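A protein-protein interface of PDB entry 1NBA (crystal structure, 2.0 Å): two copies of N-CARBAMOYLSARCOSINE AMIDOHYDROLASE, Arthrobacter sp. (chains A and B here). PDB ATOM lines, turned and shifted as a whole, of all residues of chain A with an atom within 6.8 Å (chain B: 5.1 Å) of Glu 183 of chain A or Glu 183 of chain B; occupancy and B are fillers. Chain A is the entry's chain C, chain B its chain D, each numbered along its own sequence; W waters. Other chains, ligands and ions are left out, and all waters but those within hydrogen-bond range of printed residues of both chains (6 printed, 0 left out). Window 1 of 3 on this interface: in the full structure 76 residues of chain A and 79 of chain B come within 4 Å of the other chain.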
ATOM      1  N   ARG A 146      28.178 -11.148  25.986  1.00  0.00           N
ATOM      2  CA  ARG A 146      27.212 -12.237  26.096  1.00  0.00           C
ATOM      3  C   ARG A 146      27.911 -13.542  25.719  1.00  0.00           C
ATOM      4  O   ARG A 146      28.969 -13.502  25.100  1.00  0.00           O
ATOM      5  CB  ARG A 146      26.022 -11.967  25.149  1.00  0.00           C
ATOM      6  CG  ARG A 146      25.157 -10.730  25.417  1.00  0.00           C
ATOM      7  CD  ARG A 146      24.464 -10.786  26.783  1.00  0.00           C
ATOM      8  NE  ARG A 146      24.848  -9.594  27.505  1.00  0.00           N
ATOM      9  CZ  ARG A 146      24.124  -8.491  27.531  1.00  0.00           C
ATOM     10  NH1 ARG A 146      22.965  -8.364  26.910  1.00  0.00           N
ATOM     11  NH2 ARG A 146      24.627  -7.457  28.152  1.00  0.00           N
ATOM     12  N   ALA A 147      27.314 -14.703  25.987  1.00  0.00           N
ATOM     13  CA  ALA A 147      27.925 -16.009  25.708  1.00  0.00           C
ATOM     14  C   ALA A 147      28.564 -16.241  24.340  1.00  0.00           C
ATOM     15  O   ALA A 147      29.752 -16.540  24.216  1.00  0.00           O
ATOM     16  CB  ALA A 147      26.881 -17.100  25.920  1.00  0.00           C
ATOM     17  N   SER A 148      27.783 -16.105  23.270  1.00  0.00           N
ATOM     18  CA  SER A 148      28.355 -16.290  21.950  1.00  0.00           C
ATOM     19  C   SER A 148      29.241 -15.084  21.670  1.00  0.00           C
ATOM     20  O   SER A 148      28.962 -13.953  22.093  1.00  0.00           O
ATOM     21  CB  SER A 148      27.269 -16.341  20.907  1.00  0.00           C
ATOM     22  OG  SER A 148      27.734 -16.231  19.565  1.00  0.00           O
ATOM     23  N   PHE A 150      29.313 -13.649  18.899  1.00  0.00           N
ATOM     24  CA  PHE A 150      28.705 -12.794  17.898  1.00  0.00           C
ATOM     25  C   PHE A 150      27.880 -11.626  18.452  1.00  0.00           C
ATOM     26  O   PHE A 150      28.131 -10.498  18.021  1.00  0.00           O
ATOM     27  CB  PHE A 150      27.856 -13.668  16.950  1.00  0.00           C
ATOM     28  CG  PHE A 150      28.663 -14.521  15.977  1.00  0.00           C
ATOM     29  CD1 PHE A 150      29.034 -14.007  14.748  1.00  0.00           C
ATOM     30  CD2 PHE A 150      29.025 -15.798  16.321  1.00  0.00           C
ATOM     31  CE1 PHE A 150      29.768 -14.763  13.860  1.00  0.00           C
ATOM     32  CE2 PHE A 150      29.755 -16.548  15.434  1.00  0.00           C
ATOM     33  CZ  PHE A 150      30.129 -16.041  14.206  1.00  0.00           C
ATOM     34  N   ALA A 175      29.751 -25.881  28.032  1.00  0.00           N
ATOM     35  CA  ALA A 175      28.380 -25.663  28.450  1.00  0.00           C
ATOM     36  C   ALA A 175      27.929 -24.207  28.435  1.00  0.00           C
ATOM     37  O   ALA A 175      26.860 -23.880  28.962  1.00  0.00           O
ATOM     38  CB  ALA A 175      28.183 -26.195  29.867  1.00  0.00           C
ATOM     39  N   GLY A 176      28.652 -23.328  27.770  1.00  0.00           N
ATOM     40  CA  GLY A 176      28.339 -21.925  27.780  1.00  0.00           C
ATOM     41  C   GLY A 176      28.787 -21.274  26.496  1.00  0.00           C
ATOM     42  O   GLY A 176      28.250 -21.525  25.409  1.00  0.00           O
ATOM     43  N   VAL A 178      31.363 -21.649  24.357  1.00  0.00           N
ATOM     44  CA  VAL A 178      31.775 -22.367  23.151  1.00  0.00           C
ATOM     45  C   VAL A 178      30.533 -22.857  22.410  1.00  0.00           C
ATOM     46  O   VAL A 178      30.443 -22.553  21.210  1.00  0.00           O
ATOM     47  CB  VAL A 178      32.711 -23.587  23.460  1.00  0.00           C
ATOM     48  CG1 VAL A 178      33.104 -24.388  22.216  1.00  0.00           C
ATOM     49  CG2 VAL A 178      34.038 -23.030  23.962  1.00  0.00           C
ATOM     50  N   ARG A 179      29.548 -23.507  23.066  1.00  0.00           N
ATOM     51  CA  ARG A 179      28.394 -24.016  22.347  1.00  0.00           C
ATOM     52  C   ARG A 179      27.636 -22.871  21.694  1.00  0.00           C
ATOM     53  O   ARG A 179      27.467 -22.936  20.470  1.00  0.00           O
ATOM     54  CB  ARG A 179      27.392 -24.781  23.238  1.00  0.00           C
ATOM     55  CG  ARG A 179      26.545 -25.565  22.227  1.00  0.00           C
ATOM     56  CD  ARG A 179      25.096 -25.959  22.472  1.00  0.00           C
ATOM     57  NE  ARG A 179      24.972 -27.113  23.297  1.00  0.00           N
ATOM     58  CZ  ARG A 179      24.036 -28.056  23.158  1.00  0.00           C
ATOM     59  NH1 ARG A 179      23.071 -28.092  22.239  1.00  0.00           N
ATOM     60  NH2 ARG A 179      24.070 -28.982  24.081  1.00  0.00           N
ATOM     61  N   HIS A 180      27.220 -21.807  22.412  1.00  0.00           N
ATOM     62  CA  HIS A 180      26.486 -20.718  21.784  1.00  0.00           C
ATOM     63  C   HIS A 180      27.224 -20.141  20.574  1.00  0.00           C
ATOM     64  O   HIS A 180      26.579 -19.945  19.535  1.00  0.00           O
ATOM     65  CB  HIS A 180      26.188 -19.629  22.837  1.00  0.00           C
ATOM     66  CG  HIS A 180      25.076 -18.640  22.410  1.00  0.00           C
ATOM     67  ND1 HIS A 180      24.653 -17.548  23.053  1.00  0.00           N
ATOM     68  CD2 HIS A 180      24.332 -18.716  21.237  1.00  0.00           C
ATOM     69  CE1 HIS A 180      23.719 -16.984  22.311  1.00  0.00           C
ATOM     70  NE2 HIS A 180      23.533 -17.690  21.230  1.00  0.00           N
ATOM     71  N   THR A 181      28.551 -19.916  20.630  1.00  0.00           N
ATOM     72  CA  THR A 181      29.314 -19.466  19.476  1.00  0.00           C
ATOM     73  C   THR A 181      29.230 -20.429  18.294  1.00  0.00           C
ATOM     74  O   THR A 181      29.038 -19.964  17.164  1.00  0.00           O
ATOM     75  CB  THR A 181      30.805 -19.282  19.841  1.00  0.00           C
ATOM     76  OG1 THR A 181      30.829 -18.350  20.899  1.00  0.00           O
ATOM     77  CG2 THR A 181      31.655 -18.723  18.713  1.00  0.00           C
ATOM     78  N   VAL A 182      29.357 -21.750  18.492  1.00  0.00           N
ATOM     79  CA  VAL A 182      29.317 -22.690  17.371  1.00  0.00           C
ATOM     80  C   VAL A 182      27.944 -22.676  16.719  1.00  0.00           C
ATOM     81  O   VAL A 182      27.831 -22.570  15.499  1.00  0.00           O
ATOM     82  CB  VAL A 182      29.660 -24.124  17.870  1.00  0.00           C
ATOM     83  CG1 VAL A 182      29.320 -25.201  16.860  1.00  0.00           C
ATOM     84  CG2 VAL A 182      31.165 -24.191  18.080  1.00  0.00           C
ATOM     85  N   GLU A 183      26.870 -22.736  17.488  1.00  0.00           N
ATOM     86  CA  GLU A 183      25.602 -22.783  16.802  1.00  0.00           C
ATOM     87  C   GLU A 183      25.262 -21.459  16.157  1.00  0.00           C
ATOM     88  O   GLU A 183      24.664 -21.475  15.072  1.00  0.00           O
ATOM     89  CB  GLU A 183      24.551 -23.277  17.765  1.00  0.00           C
ATOM     90  CG  GLU A 183      24.587 -22.641  19.066  1.00  0.00           C
ATOM     91  CD  GLU A 183      23.999 -23.397  20.225  1.00  0.00           C
ATOM     92  OE1 GLU A 183      23.429 -24.492  20.165  1.00  0.00           O
ATOM     93  OE2 GLU A 183      24.170 -22.814  21.267  1.00  0.00           O
ATOM     94  N   ASP A 184      25.710 -20.317  16.697  1.00  0.00           N
ATOM     95  CA  ASP A 184      25.531 -19.058  15.992  1.00  0.00           C
ATOM     96  C   ASP A 184      26.273 -19.113  14.677  1.00  0.00           C
ATOM     97  O   ASP A 184      25.713 -18.764  13.637  1.00  0.00           O
ATOM     98  CB  ASP A 184      26.078 -17.865  16.761  1.00  0.00           C
ATOM     99  CG  ASP A 184      25.037 -17.201  17.644  1.00  0.00           C
ATOM    100  OD1 ASP A 184      23.875 -17.623  17.764  1.00  0.00           O
ATOM    101  OD2 ASP A 184      25.429 -16.141  18.298  1.00  0.00           O
ATOM    102  N   ALA A 185      27.512 -19.618  14.675  1.00  0.00           N
ATOM    103  CA  ALA A 185      28.320 -19.693  13.466  1.00  0.00           C
ATOM    104  C   ALA A 185      27.743 -20.502  12.323  1.00  0.00           C
ATOM    105  O   ALA A 185      27.746 -20.029  11.177  1.00  0.00           O
ATOM    106  CB  ALA A 185      29.692 -20.278  13.786  1.00  0.00           C
ATOM    107  N   ILE A 186      27.230 -21.714  12.573  1.00  0.00           N
ATOM    108  CA  ILE A 186      26.648 -22.465  11.475  1.00  0.00           C
ATOM    109  C   ILE A 186      25.384 -21.758  10.999  1.00  0.00           C
ATOM    110  O   ILE A 186      25.137 -21.699   9.795  1.00  0.00           O
ATOM    111  CB  ILE A 186      26.376 -23.922  11.925  1.00  0.00           C
ATOM    112  CG1 ILE A 186      26.075 -24.659  10.633  1.00  0.00           C
ATOM    113  CG2 ILE A 186      25.290 -24.075  12.992  1.00  0.00           C
ATOM    114  CD1 ILE A 186      25.769 -26.164  10.767  1.00  0.00           C
ATOM    115  N   ALA A 187      24.615 -21.141  11.909  1.00  0.00           N
ATOM    116  CA  ALA A 187      23.395 -20.416  11.560  1.00  0.00           C
ATOM    117  C   ALA A 187      23.746 -19.277  10.602  1.00  0.00           C
ATOM    118  O   ALA A 187      23.181 -19.170   9.506  1.00  0.00           O
ATOM    119  CB  ALA A 187      22.749 -19.841  12.817  1.00  0.00           C
ATOM    120  N   LYS A 188      24.765 -18.478  10.950  1.00  0.00           N
ATOM    121  CA  LYS A 188      25.194 -17.377  10.105  1.00  0.00           C
ATOM    122  C   LYS A 188      25.846 -17.754   8.792  1.00  0.00           C
ATOM    123  O   LYS A 188      25.891 -16.944   7.865  1.00  0.00           O
ATOM    124  CB  LYS A 188      26.170 -16.489  10.828  1.00  0.00           C
ATOM    125  CG  LYS A 188      25.540 -15.373  11.627  1.00  0.00           C
ATOM    126  CD  LYS A 188      25.288 -15.718  13.063  1.00  0.00           C
ATOM    127  CE  LYS A 188      25.219 -14.452  13.916  1.00  0.00           C
ATOM    128  NZ  LYS A 188      24.155 -13.544  13.507  1.00  0.00           N
ATOM    129  N   PRO A 192      31.681 -24.600  11.511  1.00  0.00           N
ATOM    130  CA  PRO A 192      32.369 -24.686  12.791  1.00  0.00           C
ATOM    131  C   PRO A 192      33.182 -25.972  12.992  1.00  0.00           C
ATOM    132  O   PRO A 192      32.623 -27.082  12.908  1.00  0.00           O
ATOM    133  CB  PRO A 192      31.271 -24.551  13.829  1.00  0.00           C
ATOM    134  CG  PRO A 192      30.018 -24.284  13.025  1.00  0.00           C
ATOM    135  CD  PRO A 192      30.286 -24.944  11.684  1.00  0.00           C
ATOM    136  N   ILE A 214      26.847 -30.864  20.008  1.00  0.00           N
ATOM    137  CA  ILE A 214      27.402 -30.049  18.943  1.00  0.00           C
ATOM    138  C   ILE A 214      27.698 -30.903  17.720  1.00  0.00           C
ATOM    139  O   ILE A 214      27.333 -30.522  16.605  1.00  0.00           O
ATOM    140  CB  ILE A 214      28.712 -29.339  19.426  1.00  0.00           C
ATOM    141  CG1 ILE A 214      28.329 -28.192  20.363  1.00  0.00           C
ATOM    142  CG2 ILE A 214      29.539 -28.805  18.251  1.00  0.00           C
ATOM    143  CD1 ILE A 214      29.539 -27.503  21.062  1.00  0.00           C
ATOM    144  N   PHE A 218      25.531 -29.143  15.011  1.00  0.00           N
ATOM    145  CA  PHE A 218      26.059 -27.792  14.832  1.00  0.00           C
ATOM    146  C   PHE A 218      27.470 -27.661  14.284  1.00  0.00           C
ATOM    147  O   PHE A 218      27.763 -26.685  13.589  1.00  0.00           O
ATOM    148  CB  PHE A 218      25.955 -27.060  16.179  1.00  0.00           C
ATOM    149  CG  PHE A 218      24.534 -26.972  16.741  1.00  0.00           C
ATOM    150  CD1 PHE A 218      23.555 -26.253  16.066  1.00  0.00           C
ATOM    151  CD2 PHE A 218      24.215 -27.628  17.909  1.00  0.00           C
ATOM    152  CE1 PHE A 218      22.262 -26.191  16.558  1.00  0.00           C
ATOM    153  CE2 PHE A 218      22.927 -27.563  18.396  1.00  0.00           C
ATOM    154  CZ  PHE A 218      21.950 -26.849  17.721  1.00  0.00           C
ATOM    155  N   GLY A 219      28.399 -28.588  14.509  1.00  0.00           N
ATOM    156  CA  GLY A 219      29.731 -28.436  13.946  1.00  0.00           C
ATOM    157  C   GLY A 219      30.461 -29.764  13.984  1.00  0.00           C
ATOM    158  O   GLY A 219      29.892 -30.751  14.462  1.00  0.00           O
ATOM    159  N   VAL B 178      15.285 -25.541  20.876  1.00  0.00           N
ATOM    160  CA  VAL B 178      14.913 -24.886  22.132  1.00  0.00           C
ATOM    161  C   VAL B 178      16.133 -24.257  22.812  1.00  0.00           C
ATOM    162  O   VAL B 178      16.075 -23.064  23.143  1.00  0.00           O
ATOM    163  CB  VAL B 178      14.223 -25.904  23.078  1.00  0.00           C
ATOM    164  CG1 VAL B 178      13.926 -25.311  24.442  1.00  0.00           C
ATOM    165  CG2 VAL B 178      12.888 -26.296  22.457  1.00  0.00           C
ATOM    166  N   ARG B 179      17.269 -24.964  22.963  1.00  0.00           N
ATOM    167  CA  ARG B 179      18.412 -24.365  23.634  1.00  0.00           C
ATOM    168  C   ARG B 179      18.934 -23.127  22.901  1.00  0.00           C
ATOM    169  O   ARG B 179      19.095 -22.082  23.538  1.00  0.00           O
ATOM    170  CB  ARG B 179      19.602 -25.343  23.781  1.00  0.00           C
ATOM    171  CG  ARG B 179      20.438 -24.726  24.898  1.00  0.00           C
ATOM    172  CD  ARG B 179      21.922 -24.917  24.872  1.00  0.00           C
ATOM    173  NE  ARG B 179      22.275 -26.087  25.614  1.00  0.00           N
ATOM    174  CZ  ARG B 179      23.407 -26.199  26.309  1.00  0.00           C
ATOM    175  NH1 ARG B 179      24.322 -25.249  26.437  1.00  0.00           N
ATOM    176  NH2 ARG B 179      23.645 -27.370  26.847  1.00  0.00           N
ATOM    177  N   HIS B 180      19.186 -23.180  21.588  1.00  0.00           N
ATOM    178  CA  HIS B 180      19.707 -22.041  20.872  1.00  0.00           C
ATOM    179  C   HIS B 180      18.753 -20.866  20.984  1.00  0.00           C
ATOM    180  O   HIS B 180      19.233 -19.744  21.168  1.00  0.00           O
ATOM    181  CB  HIS B 180      19.957 -22.421  19.406  1.00  0.00           C
ATOM    182  CG  HIS B 180      20.851 -21.453  18.606  1.00  0.00           C
ATOM    183  ND1 HIS B 180      21.150 -21.464  17.307  1.00  0.00           N
ATOM    184  CD2 HIS B 180      21.471 -20.340  19.124  1.00  0.00           C
ATOM    185  CE1 HIS B 180      21.904 -20.423  17.040  1.00  0.00           C
ATOM    186  NE2 HIS B 180      22.076 -19.751  18.133  1.00  0.00           N
ATOM    187  N   THR B 181      17.433 -21.074  20.927  1.00  0.00           N
ATOM    188  CA  THR B 181      16.488 -19.985  21.100  1.00  0.00           C
ATOM    189  C   THR B 181      16.631 -19.388  22.483  1.00  0.00           C
ATOM    190  O   THR B 181      16.830 -18.180  22.596  1.00  0.00           O
ATOM    191  CB  THR B 181      15.040 -20.495  20.882  1.00  0.00           C
ATOM    192  OG1 THR B 181      14.953 -20.798  19.493  1.00  0.00           O
ATOM    193  CG2 THR B 181      13.958 -19.476  21.231  1.00  0.00           C
ATOM    194  N   VAL B 182      16.622 -20.200  23.527  1.00  0.00           N
ATOM    195  CA  VAL B 182      16.704 -19.684  24.883  1.00  0.00           C
ATOM    196  C   VAL B 182      17.943 -18.821  25.059  1.00  0.00           C
ATOM    197  O   VAL B 182      17.844 -17.668  25.480  1.00  0.00           O
ATOM    198  CB  VAL B 182      16.700 -20.887  25.845  1.00  0.00           C
ATOM    199  CG1 VAL B 182      17.112 -20.536  27.261  1.00  0.00           C
ATOM    200  CG2 VAL B 182      15.270 -21.383  25.924  1.00  0.00           C
ATOM    201  N   GLU B 183      19.117 -19.290  24.659  1.00  0.00           N
ATOM    202  CA  GLU B 183      20.277 -18.477  24.940  1.00  0.00           C
ATOM    203  C   GLU B 183      20.395 -17.246  24.052  1.00  0.00           C
ATOM    204  O   GLU B 183      21.003 -16.245  24.470  1.00  0.00           O
ATOM    205  CB  GLU B 183      21.524 -19.372  24.880  1.00  0.00           C
ATOM    206  CG  GLU B 183      21.822 -20.070  23.612  1.00  0.00           C
ATOM    207  CD  GLU B 183      22.466 -21.436  23.753  1.00  0.00           C
ATOM    208  OE1 GLU B 183      23.154 -21.789  24.710  1.00  0.00           O
ATOM    209  OE2 GLU B 183      22.241 -22.183  22.832  1.00  0.00           O
ATOM    210  N   ASP B 184      19.801 -17.285  22.857  1.00  0.00           N
ATOM    211  CA  ASP B 184      19.734 -16.091  22.034  1.00  0.00           C
ATOM    212  C   ASP B 184      18.831 -15.093  22.741  1.00  0.00           C
ATOM    213  O   ASP B 184      19.158 -13.907  22.798  1.00  0.00           O
ATOM    214  CB  ASP B 184      19.141 -16.365  20.673  1.00  0.00           C
ATOM    215  CG  ASP B 184      20.162 -16.601  19.586  1.00  0.00           C
ATOM    216  OD1 ASP B 184      21.380 -16.533  19.778  1.00  0.00           O
ATOM    217  OD2 ASP B 184      19.715 -16.850  18.374  1.00  0.00           O
ATOM    218  N   ALA B 185      17.744 -15.551  23.367  1.00  0.00           N
ATOM    219  CA  ALA B 185      16.817 -14.669  24.045  1.00  0.00           C
ATOM    220  C   ALA B 185      17.443 -13.891  25.191  1.00  0.00           C
ATOM    221  O   ALA B 185      17.309 -12.666  25.244  1.00  0.00           O
ATOM    222  CB  ALA B 185      15.642 -15.463  24.613  1.00  0.00           C
ATOM    223  N   ILE B 186      18.155 -14.547  26.114  1.00  0.00           N
ATOM    224  CA  ILE B 186      18.745 -13.823  27.232  1.00  0.00           C
ATOM    225  C   ILE B 186      19.842 -12.868  26.766  1.00  0.00           C
ATOM    226  O   ILE B 186      19.985 -11.759  27.269  1.00  0.00           O
ATOM    227  CB  ILE B 186      19.286 -14.839  28.296  1.00  0.00           C
ATOM    228  CG1 ILE B 186      19.728 -14.032  29.510  1.00  0.00           C
ATOM    229  CG2 ILE B 186      20.400 -15.727  27.743  1.00  0.00           C
ATOM    230  CD1 ILE B 186      20.131 -14.880  30.716  1.00  0.00           C
ATOM    231  N   ALA B 187      20.583 -13.253  25.742  1.00  0.00           N
ATOM    232  CA  ALA B 187      21.620 -12.420  25.190  1.00  0.00           C
ATOM    233  C   ALA B 187      20.988 -11.140  24.656  1.00  0.00           C
ATOM    234  O   ALA B 187      21.427 -10.047  24.993  1.00  0.00           O
ATOM    235  CB  ALA B 187      22.319 -13.148  24.047  1.00  0.00           C
ATOM    236  N   PHE B 218      21.264 -19.742  31.464  1.00  0.00           N
ATOM    237  CA  PHE B 218      20.540 -19.054  30.408  1.00  0.00           C
ATOM    238  C   PHE B 218      19.054 -18.842  30.630  1.00  0.00           C
ATOM    239  O   PHE B 218      18.473 -18.028  29.921  1.00  0.00           O
ATOM    240  CB  PHE B 218      20.692 -19.786  29.069  1.00  0.00           C
ATOM    241  CG  PHE B 218      22.107 -20.076  28.584  1.00  0.00           C
ATOM    242  CD1 PHE B 218      22.924 -19.049  28.155  1.00  0.00           C
ATOM    243  CD2 PHE B 218      22.557 -21.382  28.573  1.00  0.00           C
ATOM    244  CE1 PHE B 218      24.199 -19.333  27.711  1.00  0.00           C
ATOM    245  CE2 PHE B 218      23.823 -21.658  28.133  1.00  0.00           C
ATOM    246  CZ  PHE B 218      24.640 -20.640  27.704  1.00  0.00           C
HETATM  247  O   HOH W   1      22.243 -22.860  15.013  1.00  0.00           O
HETATM  248  O   HOH W   2      20.534  -9.122  28.141  1.00  0.00           O
HETATM  249  O   HOH W   3      23.232 -14.784  19.319  1.00  0.00           O
HETATM  250  O   HOH W   4      23.555 -16.473  25.434  1.00  0.00           O
HETATM  251  O   HOH W   5      21.626 -16.690  16.291  1.00  0.00           O
HETATM  252  O   HOH W   6      25.796 -23.178  25.390  1.00  0.00           O
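CB of Ala 147 of chain A touches CE1 of Phe 218 of chain B, at 3.9 Å. Ala 175 of chain A touches Arg 179 of chain B (O to NH1, 3.8 Å). Phe 218 of chain B touches Ala 175 of chain A (CE2 to O, 3.9 Å). Phe 218 of chain B touches Gly 176 of chain A. His 180 of chain A touches His 180 of chain B. Glu 183 of chain B touches His 180 of chain A (O to CE1, 3.5 Å). His 180 of chain B touches Glu 183 of chain A (CE1 to O, 3.5 Å).
The backbone carbonyl oxygen (O) of Ala 187 of chain B sits at hydrogen-bond distance from the guanidinium group (NH1) of Arg 146 of chain A, at 3.0 Å. OD1 of Asp 184 of chain B is in hydrogen-bond range of NE2 of His 180 of chain A, at 2.8 Å. The side-chain carboxylate (OE2) of Glu 183 of chain B sits close to the side-chain carboxylate (OE2) of Glu 183 of chain A. The side-chain carboxylate (OD1) of Asp 184 of chain A is in hydrogen-bond range of a ring nitrogen (NE2) of His 180 of chain B (2.8 Å). NH2 of Arg 179 of chain A sits close to NH2 of Arg 179 of chain B (3.2 Å). The side-chain carboxylate (OD1) of Asp 184 of chain B sits close to the side-chain carboxylate (OD1) of Asp 184 of chain A (3.4 Å).
His 180 of chain B touches its own counterpart, His 180 of chain A. His 180 of chain A touches Glu 183 of chain B, and with the chains exchanged Glu 183 of chain A touches His 180 of chain B. His 180 of chain A touches Asp 184 of chain B, and with the chains exchanged Asp 184 of chain A touches His 180 of chain B. Glu 183 of chain B touches its own counterpart, Glu 183 of chain A. Positions printed for both chains: 178, 179, 180, 181, 182, 183, 184, 185, 186, 187 and 218.
Of the printed residues of chain B, Ala 147 of chain A touches Phe 218 (3.9 Å). Of the printed residues of chain B, Gly 176 of chain A touches Phe 218. Val 178 of chain A touches none of the printed residues of chain B. Printed residues of chain B within 4 Å of His 180 of chain A: His 180, Glu 183 and Asp 184. Glu 183 of chain A touches two residues of chain B. Ile 186 of chain A touches none of the printed residues of chain B. The nearest residue of chain B that does not touch Glu 183 of chain A is Arg 179 of chain B (4.7 Å). The nearest residue of chain A that does not touch Glu 183 of chain B is Arg 179 of chain A (4.7 Å). The nearest printed residue of chain B that does not touch Gly 176 of chain A is Arg 179 of chain B (4.9 Å).
Water W3 lies within hydrogen-bond range of the side-chain carboxylate of Asp 184 of chain B (2.6 Å), the side-chain carboxylate of Asp 184 of chain A (2.8 Å) and a ring nitrogen (NE2) of His 180 of chain A (3.5 Å). Water W4 bridges the backbone carbonyl oxygen of Glu 183 of chain B (2.7 Å) and a ring nitrogen (ND1) of His 180 of chain A (2.8 Å). Water W6 lies within hydrogen-bond range of the guanidinium group (NH1) of Arg 179 of chain B, the backbone carbonyl oxygen (O) of Gly 176 of chain A and the side-chain carboxylate (OE1) of Glu 183 of chain B. Water W1 bridges the backbone carbonyl oxygen (O) of Glu 183 of chain A (2.8 Å) and a ring nitrogen (ND1) of His 180 of chain B (2.9 Å). Water W2 lies within hydrogen-bond range of NH1 of Arg 146 of chain A (2.8 Å), O of Ile 186 of chain B (2.8 Å) and O of Ala 187 of chain B (3.4 Å). Water W5 lies within hydrogen-bond range of the side-chain carboxylate of Asp 184 of chain B (2.8 Å) and the side-chain carboxylate of Asp 184 of chain A (2.8 Å).
The backbone NH (N) of Ser 148 of chain A lies within hydrogen-bond range of a ring nitrogen (ND1) of His 180 of chain A, at 3.5 Å. The side-chain hydroxyl of Ser 148 of chain A lies within hydrogen-bond range of the side-chain carboxylate of Asp 184 of chain A, at 2.6 Å. The backbone NH (N) of His 180 of chain A sits close to the side-chain carboxylate (OE2) of Glu 183 of chain A (3.4 Å). NE2 of His 180 of chain A is in hydrogen-bond range of OD1 of Asp 184 of chain A, 3.5 Å away. The backbone NH of His 180 of chain B lies close to the side-chain carboxylate of Glu 183 of chain B.
Hydrophobic or aromatic side chains of chain B within 4 Å of the printed part of chain A: His 180, Ala 187 and Phe 218. Hydrophobic or aromatic side chains of chain A within 4 Å of the printed part of chain B: Ala 147 and His 180.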
